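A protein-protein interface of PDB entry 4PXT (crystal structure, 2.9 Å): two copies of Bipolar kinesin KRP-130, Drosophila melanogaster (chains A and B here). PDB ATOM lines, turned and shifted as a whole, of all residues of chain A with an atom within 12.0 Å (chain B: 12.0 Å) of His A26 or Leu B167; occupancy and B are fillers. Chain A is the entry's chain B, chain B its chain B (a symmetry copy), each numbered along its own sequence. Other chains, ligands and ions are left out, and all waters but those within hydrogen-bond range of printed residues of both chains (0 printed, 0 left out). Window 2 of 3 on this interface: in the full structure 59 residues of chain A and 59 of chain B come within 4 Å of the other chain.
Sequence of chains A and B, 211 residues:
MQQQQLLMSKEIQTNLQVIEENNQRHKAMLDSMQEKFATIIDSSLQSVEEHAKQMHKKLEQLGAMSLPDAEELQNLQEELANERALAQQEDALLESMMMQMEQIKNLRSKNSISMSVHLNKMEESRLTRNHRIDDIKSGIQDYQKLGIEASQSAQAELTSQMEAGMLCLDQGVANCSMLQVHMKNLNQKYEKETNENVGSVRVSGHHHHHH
The backbone carbonyl oxygen of Ala B164 lies close to the side-chain sulfur of Met A29 (3.5 Å).
A ring nitrogen (NE2) of His A26 sits at hydrogen-bond distance from the side-chain amide oxygen (OD1) of Asn A22 (2.9 Å).
The side-chain hydroxyl of Ser A32 sits at hydrogen-bond distance from the backbone carbonyl oxygen of Ala A28.
The side-chain hydroxyl of Ser A32 lies within hydrogen-bond range of the backbone carbonyl oxygen of Met A29 (3.4 Å).
Among the printed residues, merely in contact across the chains: His A26 with Leu B167 (3.9 Å), Ser A32 with Gln B161 (3.8 Å), Met A33 with Gln B161 (3.8 Å) and Met A33 with Met B162 (3.5 Å).
Val A18 touches none of the printed residues of chain B.
Asn A22 touches none of the printed residues of chain B.
No residue of chain B comes within 4 Å of Asn A23.
No residue of chain B comes within 4 Å of Ala A28.
Of chain B, only Ala B164 (3.5 Å) comes within 4 Å of Met A29.
No residue of chain B comes within 4 Å of Leu A30.
Of the printed residues of chain B, Ser A32 touches Gln B161 (3.8 Å).
Printed residues of chain B within 4 Å of Met A33: Gln B161 and Met B162.
Gln A34 touches none of the printed residues of chain B.
Of the printed residues of chain A, Gln B161 touches Ser A32 (3.8 Å) and Met A33 (3.8 Å).
Printed residues of chain A within 4 Å of Met B162: Met A33 (3.5 Å).
Of the printed residues of chain A, Ala B164 touches Met A29.
No residue of chain A comes within 4 Å of Met B166.
Of chain A, only His A26 (3.9 Å) comes within 4 Å of Leu B167.
The nearest residue of chain A that does not touch Leu B167 is Asn A22 (4.5 Å).
Printed residues of chain A that touch a printed residue of chain B: His A26, Met A29, Ser A32 and Met A33.
Hydrophobic or aromatic side chains of chain A that line the printed part of chain B: His A26, Met A29 and Met A33.
Of the 11 printed residues of chain B, 4 touch a printed residue of chain A.
Among the printed residues, no Asp or Glu carboxylate lies within 4 Å of a Lys or Arg side-chain nitrogen of the other chain.
No position is printed for both chains.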
ATOM      1  N   VAL A  18     -19.539  -1.314 -29.329  1.00  0.00           N
ATOM      2  CA  VAL A  18     -19.876  -2.453 -28.478  1.00  0.00           C
ATOM      3  C   VAL A  18     -18.754  -3.494 -28.504  1.00  0.00           C
ATOM      4  O   VAL A  18     -18.890  -4.595 -27.971  1.00  0.00           O
ATOM      5  CB  VAL A  18     -21.215  -3.098 -28.918  1.00  0.00           C
ATOM      6  CG1 VAL A  18     -21.912  -3.792 -27.742  1.00  0.00           C
ATOM      7  CG2 VAL A  18     -22.126  -2.048 -29.557  1.00  0.00           C
ATOM      8  N   ILE A  19     -17.639  -3.132 -29.135  1.00  0.00           N
ATOM      9  CA  ILE A  19     -16.406  -3.903 -29.031  1.00  0.00           C
ATOM     10  C   ILE A  19     -15.902  -3.812 -27.590  1.00  0.00           C
ATOM     11  O   ILE A  19     -15.088  -4.623 -27.151  1.00  0.00           O
ATOM     12  CB  ILE A  19     -15.325  -3.401 -30.021  1.00  0.00           C
ATOM     13  CG1 ILE A  19     -14.201  -4.429 -30.174  1.00  0.00           C
ATOM     14  CG2 ILE A  19     -14.768  -2.060 -29.577  1.00  0.00           C
ATOM     15  CD1 ILE A  19     -13.074  -3.974 -31.078  1.00  0.00           C
ATOM     16  N   GLU A  20     -16.407  -2.819 -26.857  1.00  0.00           N
ATOM     17  CA  GLU A  20     -16.150  -2.688 -25.426  1.00  0.00           C
ATOM     18  C   GLU A  20     -16.797  -3.845 -24.662  1.00  0.00           C
ATOM     19  O   GLU A  20     -16.274  -4.287 -23.640  1.00  0.00           O
ATOM     20  CB  GLU A  20     -16.670  -1.342 -24.903  1.00  0.00           C
ATOM     21  CG  GLU A  20     -16.583  -1.163 -23.384  1.00  0.00           C
ATOM     22  CD  GLU A  20     -17.825  -1.650 -22.650  1.00  0.00           C
ATOM     23  OE1 GLU A  20     -18.829  -1.960 -23.324  1.00  0.00           O
ATOM     24  OE2 GLU A  20     -17.794  -1.734 -21.402  1.00  0.00           O
ATOM     25  N   GLU A  21     -17.928  -4.332 -25.170  1.00  0.00           N
ATOM     26  CA  GLU A  21     -18.680  -5.416 -24.535  1.00  0.00           C
ATOM     27  C   GLU A  21     -17.846  -6.689 -24.406  1.00  0.00           C
ATOM     28  O   GLU A  21     -17.995  -7.446 -23.445  1.00  0.00           O
ATOM     29  CB  GLU A  21     -19.954  -5.718 -25.338  1.00  0.00           C
ATOM     30  CG  GLU A  21     -20.814  -6.872 -24.823  1.00  0.00           C
ATOM     31  CD  GLU A  21     -21.443  -6.598 -23.469  1.00  0.00           C
ATOM     32  OE1 GLU A  21     -21.477  -5.422 -23.049  1.00  0.00           O
ATOM     33  OE2 GLU A  21     -21.902  -7.565 -22.823  1.00  0.00           O
ATOM     34  N   ASN A  22     -16.977  -6.925 -25.382  1.00  0.00           N
ATOM     35  CA  ASN A  22     -16.046  -8.045 -25.328  1.00  0.00           C
ATOM     36  C   ASN A  22     -14.988  -7.814 -24.245  1.00  0.00           C
ATOM     37  O   ASN A  22     -14.603  -8.743 -23.531  1.00  0.00           O
ATOM     38  CB  ASN A  22     -15.384  -8.274 -26.692  1.00  0.00           C
ATOM     39  CG  ASN A  22     -14.695  -9.632 -26.794  1.00  0.00           C
ATOM     40  OD1 ASN A  22     -14.908 -10.521 -25.964  1.00  0.00           O
ATOM     41  ND2 ASN A  22     -13.865  -9.796 -27.820  1.00  0.00           N
ATOM     42  N   ASN A  23     -14.530  -6.570 -24.126  1.00  0.00           N
ATOM     43  CA  ASN A  23     -13.572  -6.186 -23.090  1.00  0.00           C
ATOM     44  C   ASN A  23     -14.148  -6.334 -21.687  1.00  0.00           C
ATOM     45  O   ASN A  23     -13.481  -6.840 -20.785  1.00  0.00           O
ATOM     46  CB  ASN A  23     -13.117  -4.740 -23.295  1.00  0.00           C
ATOM     47  CG  ASN A  23     -12.425  -4.521 -24.625  1.00  0.00           C
ATOM     48  OD1 ASN A  23     -12.282  -5.447 -25.423  1.00  0.00           O
ATOM     49  ND2 ASN A  23     -12.010  -3.285 -24.880  1.00  0.00           N
ATOM     50  N   GLN A  24     -15.390  -5.892 -21.514  1.00  0.00           N
ATOM     51  CA  GLN A  24     -16.055  -5.943 -20.219  1.00  0.00           C
ATOM     52  C   GLN A  24     -16.242  -7.365 -19.693  1.00  0.00           C
ATOM     53  O   GLN A  24     -16.133  -7.602 -18.490  1.00  0.00           O
ATOM     54  CB  GLN A  24     -17.410  -5.230 -20.290  1.00  0.00           C
ATOM     55  CG  GLN A  24     -18.176  -5.208 -18.974  1.00  0.00           C
ATOM     56  CD  GLN A  24     -17.424  -4.502 -17.858  1.00  0.00           C
ATOM     57  OE1 GLN A  24     -17.118  -3.313 -17.956  1.00  0.00           O
ATOM     58  NE2 GLN A  24     -17.137  -5.231 -16.784  1.00  0.00           N
ATOM     59  N   ARG A  25     -16.516  -8.318 -20.579  1.00  0.00           N
ATOM     60  CA  ARG A  25     -16.624  -9.704 -20.137  1.00  0.00           C
ATOM     61  C   ARG A  25     -15.239 -10.288 -19.881  1.00  0.00           C
ATOM     62  O   ARG A  25     -15.049 -11.086 -18.962  1.00  0.00           O
ATOM     63  CB  ARG A  25     -17.375 -10.553 -21.157  1.00  0.00           C
ATOM     64  CG  ARG A  25     -17.406 -12.039 -20.827  1.00  0.00           C
ATOM     65  CD  ARG A  25     -18.502 -12.760 -21.601  1.00  0.00           C
ATOM     66  NE  ARG A  25     -19.851 -12.388 -21.178  1.00  0.00           N
ATOM     67  CZ  ARG A  25     -20.610 -11.468 -21.769  1.00  0.00           C
ATOM     68  NH1 ARG A  25     -20.142 -10.784 -22.803  1.00  0.00           N
ATOM     69  NH2 ARG A  25     -21.827 -11.206 -21.307  1.00  0.00           N
ATOM     70  N   HIS A  26     -14.270  -9.877 -20.695  1.00  0.00           N
ATOM     71  CA  HIS A  26     -12.882 -10.264 -20.484  1.00  0.00           C
ATOM     72  C   HIS A  26     -12.346  -9.700 -19.167  1.00  0.00           C
ATOM     73  O   HIS A  26     -11.678 -10.403 -18.411  1.00  0.00           O
ATOM     74  CB  HIS A  26     -12.012  -9.799 -21.652  1.00  0.00           C
ATOM     75  CG  HIS A  26     -12.212 -10.587 -22.910  1.00  0.00           C
ATOM     76  ND1 HIS A  26     -11.426 -10.415 -24.029  1.00  0.00           N
ATOM     77  CD2 HIS A  26     -13.104 -11.557 -23.221  1.00  0.00           C
ATOM     78  CE1 HIS A  26     -11.829 -11.241 -24.978  1.00  0.00           C
ATOM     79  NE2 HIS A  26     -12.846 -11.946 -24.513  1.00  0.00           N
ATOM     80  N   LYS A  27     -12.638  -8.433 -18.889  1.00  0.00           N
ATOM     81  CA  LYS A  27     -12.232  -7.832 -17.624  1.00  0.00           C
ATOM     82  C   LYS A  27     -12.968  -8.484 -16.455  1.00  0.00           C
ATOM     83  O   LYS A  27     -12.435  -8.577 -15.349  1.00  0.00           O
ATOM     84  CB  LYS A  27     -12.480  -6.324 -17.643  1.00  0.00           C
ATOM     85  CG  LYS A  27     -11.775  -5.560 -16.533  1.00  0.00           C
ATOM     86  CD  LYS A  27     -12.300  -4.134 -16.435  1.00  0.00           C
ATOM     87  CE  LYS A  27     -12.358  -3.461 -17.803  1.00  0.00           C
ATOM     88  NZ  LYS A  27     -12.996  -2.113 -17.737  1.00  0.00           N
ATOM     89  N   ALA A  28     -14.193  -8.939 -16.711  1.00  0.00           N
ATOM     90  CA  ALA A  28     -14.996  -9.638 -15.711  1.00  0.00           C
ATOM     91  C   ALA A  28     -14.440 -11.034 -15.444  1.00  0.00           C
ATOM     92  O   ALA A  28     -14.721 -11.642 -14.411  1.00  0.00           O
ATOM     93  CB  ALA A  28     -16.450  -9.725 -16.153  1.00  0.00           C
ATOM     94  N   MET A  29     -13.643 -11.527 -16.387  1.00  0.00           N
ATOM     95  CA  MET A  29     -13.053 -12.856 -16.293  1.00  0.00           C
ATOM     96  C   MET A  29     -11.848 -12.838 -15.356  1.00  0.00           C
ATOM     97  O   MET A  29     -11.402 -13.883 -14.891  1.00  0.00           O
ATOM     98  CB  MET A  29     -12.643 -13.360 -17.682  1.00  0.00           C
ATOM     99  CG  MET A  29     -12.373 -14.853 -17.773  1.00  0.00           C
ATOM    100  SD  MET A  29     -13.946 -15.920 -17.333  1.00  0.00           S
ATOM    101  CE  MET A  29     -15.277 -14.986 -18.411  1.00  0.00           C
ATOM    102  N   LEU A  30     -11.328 -11.646 -15.077  1.00  0.00           N
ATOM    103  CA  LEU A  30     -10.164 -11.512 -14.211  1.00  0.00           C
ATOM    104  C   LEU A  30     -10.595 -11.310 -12.766  1.00  0.00           C
ATOM    105  O   LEU A  30     -10.040 -11.922 -11.851  1.00  0.00           O
ATOM    106  CB  LEU A  30      -9.286 -10.341 -14.653  1.00  0.00           C
ATOM    107  CG  LEU A  30      -8.744 -10.331 -16.083  1.00  0.00           C
ATOM    108  CD1 LEU A  30      -7.592  -9.343 -16.190  1.00  0.00           C
ATOM    109  CD2 LEU A  30      -8.315 -11.721 -16.539  1.00  0.00           C
ATOM    110  N   ASP A  31     -11.593 -10.458 -12.560  1.00  0.00           N
ATOM    111  CA  ASP A  31     -12.070 -10.162 -11.215  1.00  0.00           C
ATOM    112  C   ASP A  31     -12.853 -11.327 -10.608  1.00  0.00           C
ATOM    113  O   ASP A  31     -13.027 -11.401  -9.389  1.00  0.00           O
ATOM    114  CB  ASP A  31     -12.923  -8.895 -11.226  1.00  0.00           C
ATOM    115  CG  ASP A  31     -12.139  -7.681 -11.673  1.00  0.00           C
ATOM    116  OD1 ASP A  31     -12.256  -7.297 -12.855  1.00  0.00           O
ATOM    117  OD2 ASP A  31     -11.394  -7.117 -10.842  1.00  0.00           O
ATOM    118  N   SER A  32     -13.325 -12.232 -11.460  1.00  0.00           N
ATOM    119  CA  SER A  32     -13.943 -13.475 -11.004  1.00  0.00           C
ATOM    120  C   SER A  32     -12.865 -14.522 -10.774  1.00  0.00           C
ATOM    121  O   SER A  32     -13.101 -15.573 -10.168  1.00  0.00           O
ATOM    122  CB  SER A  32     -14.963 -13.980 -12.022  1.00  0.00           C
ATOM    123  OG  SER A  32     -14.341 -14.251 -13.270  1.00  0.00           O
ATOM    124  N   MET A  33     -11.674 -14.214 -11.274  1.00  0.00           N
ATOM    125  CA  MET A  33     -10.526 -15.095 -11.179  1.00  0.00           C
ATOM    126  C   MET A  33      -9.587 -14.669 -10.067  1.00  0.00           C
ATOM    127  O   MET A  33      -9.093 -15.508  -9.316  1.00  0.00           O
ATOM    128  CB  MET A  33      -9.781 -15.124 -12.501  1.00  0.00           C
ATOM    129  CG  MET A  33      -8.453 -15.828 -12.443  1.00  0.00           C
ATOM    130  SD  MET A  33      -7.844 -16.149 -14.247  1.00  0.00           S
ATOM    131  CE  MET A  33      -9.597 -16.399 -15.066  1.00  0.00           C
ATOM    132  N   GLN A  34      -9.317 -13.368  -9.978  1.00  0.00           N
ATOM    133  CA  GLN A  34      -8.465 -12.852  -8.912  1.00  0.00           C
ATOM    134  C   GLN A  34      -9.067 -13.208  -7.556  1.00  0.00           C
ATOM    135  O   GLN A  34      -8.347 -13.387  -6.574  1.00  0.00           O
ATOM    136  CB  GLN A  34      -8.267 -11.335  -9.020  1.00  0.00           C
ATOM    137  CG  GLN A  34      -7.153 -10.814  -8.107  1.00  0.00           C
ATOM    138  CD  GLN A  34      -7.193  -9.307  -7.888  1.00  0.00           C
ATOM    139  OE1 GLN A  34      -7.601  -8.542  -8.767  1.00  0.00           O
ATOM    140  NE2 GLN A  34      -6.765  -8.875  -6.704  1.00  0.00           N
ATOM    141  N   GLU A  35     -10.392 -13.330  -7.516  1.00  0.00           N
ATOM    142  CA  GLU A  35     -11.094 -13.675  -6.287  1.00  0.00           C
ATOM    143  C   GLU A  35     -10.945 -15.154  -5.942  1.00  0.00           C
ATOM    144  O   GLU A  35     -10.648 -15.500  -4.799  1.00  0.00           O
ATOM    145  CB  GLU A  35     -12.577 -13.320  -6.408  1.00  0.00           C
ATOM    146  CG  GLU A  35     -12.921 -11.962  -5.831  1.00  0.00           C
ATOM    147  CD  GLU A  35     -12.359 -11.770  -4.436  1.00  0.00           C
ATOM    148  OE1 GLU A  35     -12.664 -12.598  -3.551  1.00  0.00           O
ATOM    149  OE2 GLU A  35     -11.594 -10.803  -4.228  1.00  0.00           O
ATOM    150  N   SER B 160     -10.685 -24.731 -14.062  1.00  0.00           N
ATOM    151  CA  SER B 160     -12.100 -24.440 -14.272  1.00  0.00           C
ATOM    152  C   SER B 160     -12.291 -22.990 -14.693  1.00  0.00           C
ATOM    153  O   SER B 160     -13.282 -22.653 -15.334  1.00  0.00           O
ATOM    154  CB  SER B 160     -12.917 -24.696 -13.023  1.00  0.00           C
ATOM    155  OG  SER B 160     -13.205 -23.460 -12.382  1.00  0.00           O
ATOM    156  N   GLN B 161     -11.381 -22.119 -14.283  1.00  0.00           N
ATOM    157  CA  GLN B 161     -11.411 -20.741 -14.745  1.00  0.00           C
ATOM    158  C   GLN B 161     -10.898 -20.650 -16.184  1.00  0.00           C
ATOM    159  O   GLN B 161     -11.358 -19.816 -16.962  1.00  0.00           O
ATOM    160  CB  GLN B 161     -10.606 -19.825 -13.825  1.00  0.00           C
ATOM    161  CG  GLN B 161     -11.117 -19.759 -12.387  1.00  0.00           C
ATOM    162  CD  GLN B 161     -12.365 -18.905 -12.241  1.00  0.00           C
ATOM    163  OE1 GLN B 161     -12.616 -18.000 -13.040  1.00  0.00           O
ATOM    164  NE2 GLN B 161     -13.155 -19.190 -11.210  1.00  0.00           N
ATOM    165  N   MET B 162      -9.948 -21.517 -16.530  1.00  0.00           N
ATOM    166  CA  MET B 162      -9.391 -21.576 -17.881  1.00  0.00           C
ATOM    167  C   MET B 162     -10.360 -22.158 -18.896  1.00  0.00           C
ATOM    168  O   MET B 162     -10.390 -21.752 -20.058  1.00  0.00           O
ATOM    169  CB  MET B 162      -8.124 -22.428 -17.876  1.00  0.00           C
ATOM    170  CG  MET B 162      -7.052 -21.920 -16.940  1.00  0.00           C
ATOM    171  SD  MET B 162      -6.602 -20.060 -17.274  1.00  0.00           S
ATOM    172  CE  MET B 162      -7.554 -19.236 -15.790  1.00  0.00           C
ATOM    173  N   GLU B 163     -11.156 -23.116 -18.443  1.00  0.00           N
ATOM    174  CA  GLU B 163     -12.138 -23.754 -19.296  1.00  0.00           C
ATOM    175  C   GLU B 163     -13.232 -22.759 -19.638  1.00  0.00           C
ATOM    176  O   GLU B 163     -13.757 -22.756 -20.753  1.00  0.00           O
ATOM    177  CB  GLU B 163     -12.718 -24.980 -18.591  1.00  0.00           C
ATOM    178  CG  GLU B 163     -13.600 -25.873 -19.443  1.00  0.00           C
ATOM    179  CD  GLU B 163     -14.007 -27.132 -18.700  1.00  0.00           C
ATOM    180  OE1 GLU B 163     -13.625 -27.268 -17.516  1.00  0.00           O
ATOM    181  OE2 GLU B 163     -14.706 -27.982 -19.291  1.00  0.00           O
ATOM    182  N   ALA B 164     -13.558 -21.904 -18.671  1.00  0.00           N
ATOM    183  CA  ALA B 164     -14.588 -20.894 -18.863  1.00  0.00           C
ATOM    184  C   ALA B 164     -14.081 -19.638 -19.573  1.00  0.00           C
ATOM    185  O   ALA B 164     -14.727 -18.596 -19.513  1.00  0.00           O
ATOM    186  CB  ALA B 164     -15.200 -20.518 -17.517  1.00  0.00           C
ATOM    187  N   GLY B 165     -12.920 -19.711 -20.218  1.00  0.00           N
ATOM    188  CA  GLY B 165     -12.437 -18.556 -20.953  1.00  0.00           C
ATOM    189  C   GLY B 165     -12.799 -18.627 -22.427  1.00  0.00           C
ATOM    190  O   GLY B 165     -12.154 -17.987 -23.253  1.00  0.00           O
ATOM    191  N   MET B 166     -13.824 -19.417 -22.756  1.00  0.00           N
ATOM    192  CA  MET B 166     -14.249 -19.568 -24.149  1.00  0.00           C
ATOM    193  C   MET B 166     -15.339 -18.569 -24.559  1.00  0.00           C
ATOM    194  O   MET B 166     -15.854 -17.853 -23.717  1.00  0.00           O
ATOM    195  CB  MET B 166     -14.819 -20.977 -24.331  1.00  0.00           C
ATOM    196  CG  MET B 166     -13.871 -22.093 -24.026  1.00  0.00           C
ATOM    197  SD  MET B 166     -14.696 -23.796 -24.472  1.00  0.00           S
ATOM    198  CE  MET B 166     -13.322 -24.964 -23.748  1.00  0.00           C
ATOM    199  N   LEU B 167     -15.710 -18.521 -25.837  1.00  0.00           N
ATOM    200  CA  LEU B 167     -16.663 -17.510 -26.267  1.00  0.00           C
ATOM    201  C   LEU B 167     -17.765 -18.268 -27.065  1.00  0.00           C
ATOM    202  O   LEU B 167     -18.533 -19.030 -26.485  1.00  0.00           O
ATOM    203  CB  LEU B 167     -15.944 -16.469 -27.139  1.00  0.00           C
ATOM    204  CG  LEU B 167     -14.793 -15.654 -26.521  1.00  0.00           C
ATOM    205  CD1 LEU B 167     -14.314 -14.642 -27.546  1.00  0.00           C
ATOM    206  CD2 LEU B 167     -15.172 -14.987 -25.230  1.00  0.00           C
ATOM    207  N   CYS B 168     -17.827 -18.037 -28.391  1.00  0.00           N
ATOM    208  CA  CYS B 168     -18.915 -18.520 -29.281  1.00  0.00           C
ATOM    209  C   CYS B 168     -18.173 -19.142 -30.507  1.00  0.00           C
ATOM    210  O   CYS B 168     -17.115 -18.637 -30.877  1.00  0.00           O
ATOM    211  CB  CYS B 168     -19.975 -17.454 -29.655  1.00  0.00           C
ATOM    212  SG  CYS B 168     -19.485 -15.859 -30.342  1.00  0.00           S
ATOM    213  N   LEU B 169     -18.651 -20.227 -31.125  1.00  0.00           N
ATOM    214  CA  LEU B 169     -19.819 -20.993 -30.765  1.00  0.00           C
ATOM    215  C   LEU B 169     -19.330 -22.305 -30.203  1.00  0.00           C
ATOM    216  O   LEU B 169     -18.211 -22.749 -30.500  1.00  0.00           O
ATOM    217  CB  LEU B 169     -20.744 -21.228 -31.986  1.00  0.00           C
ATOM    218  CG  LEU B 169     -20.393 -21.849 -33.364  1.00  0.00           C
ATOM    219  CD1 LEU B 169     -19.264 -22.885 -33.369  1.00  0.00           C
ATOM    220  CD2 LEU B 169     -21.646 -22.451 -34.004  1.00  0.00           C
ATOM    221  N   ASP B 170     -20.163 -22.896 -29.361  1.00  0.00           N
ATOM    222  CA  ASP B 170     -19.922 -24.212 -28.812  1.00  0.00           C
ATOM    223  C   ASP B 170     -18.586 -24.286 -28.072  1.00  0.00           C
ATOM    224  O   ASP B 170     -18.019 -25.365 -27.894  1.00  0.00           O
ATOM    225  CB  ASP B 170     -19.971 -25.247 -29.931  1.00  0.00           C
ATOM    226  CG  ASP B 170     -21.365 -25.390 -30.524  1.00  0.00           C
ATOM    227  OD1 ASP B 170     -22.347 -25.054 -29.825  1.00  0.00           O
ATOM    228  OD2 ASP B 170     -21.482 -25.855 -31.678  1.00  0.00           O
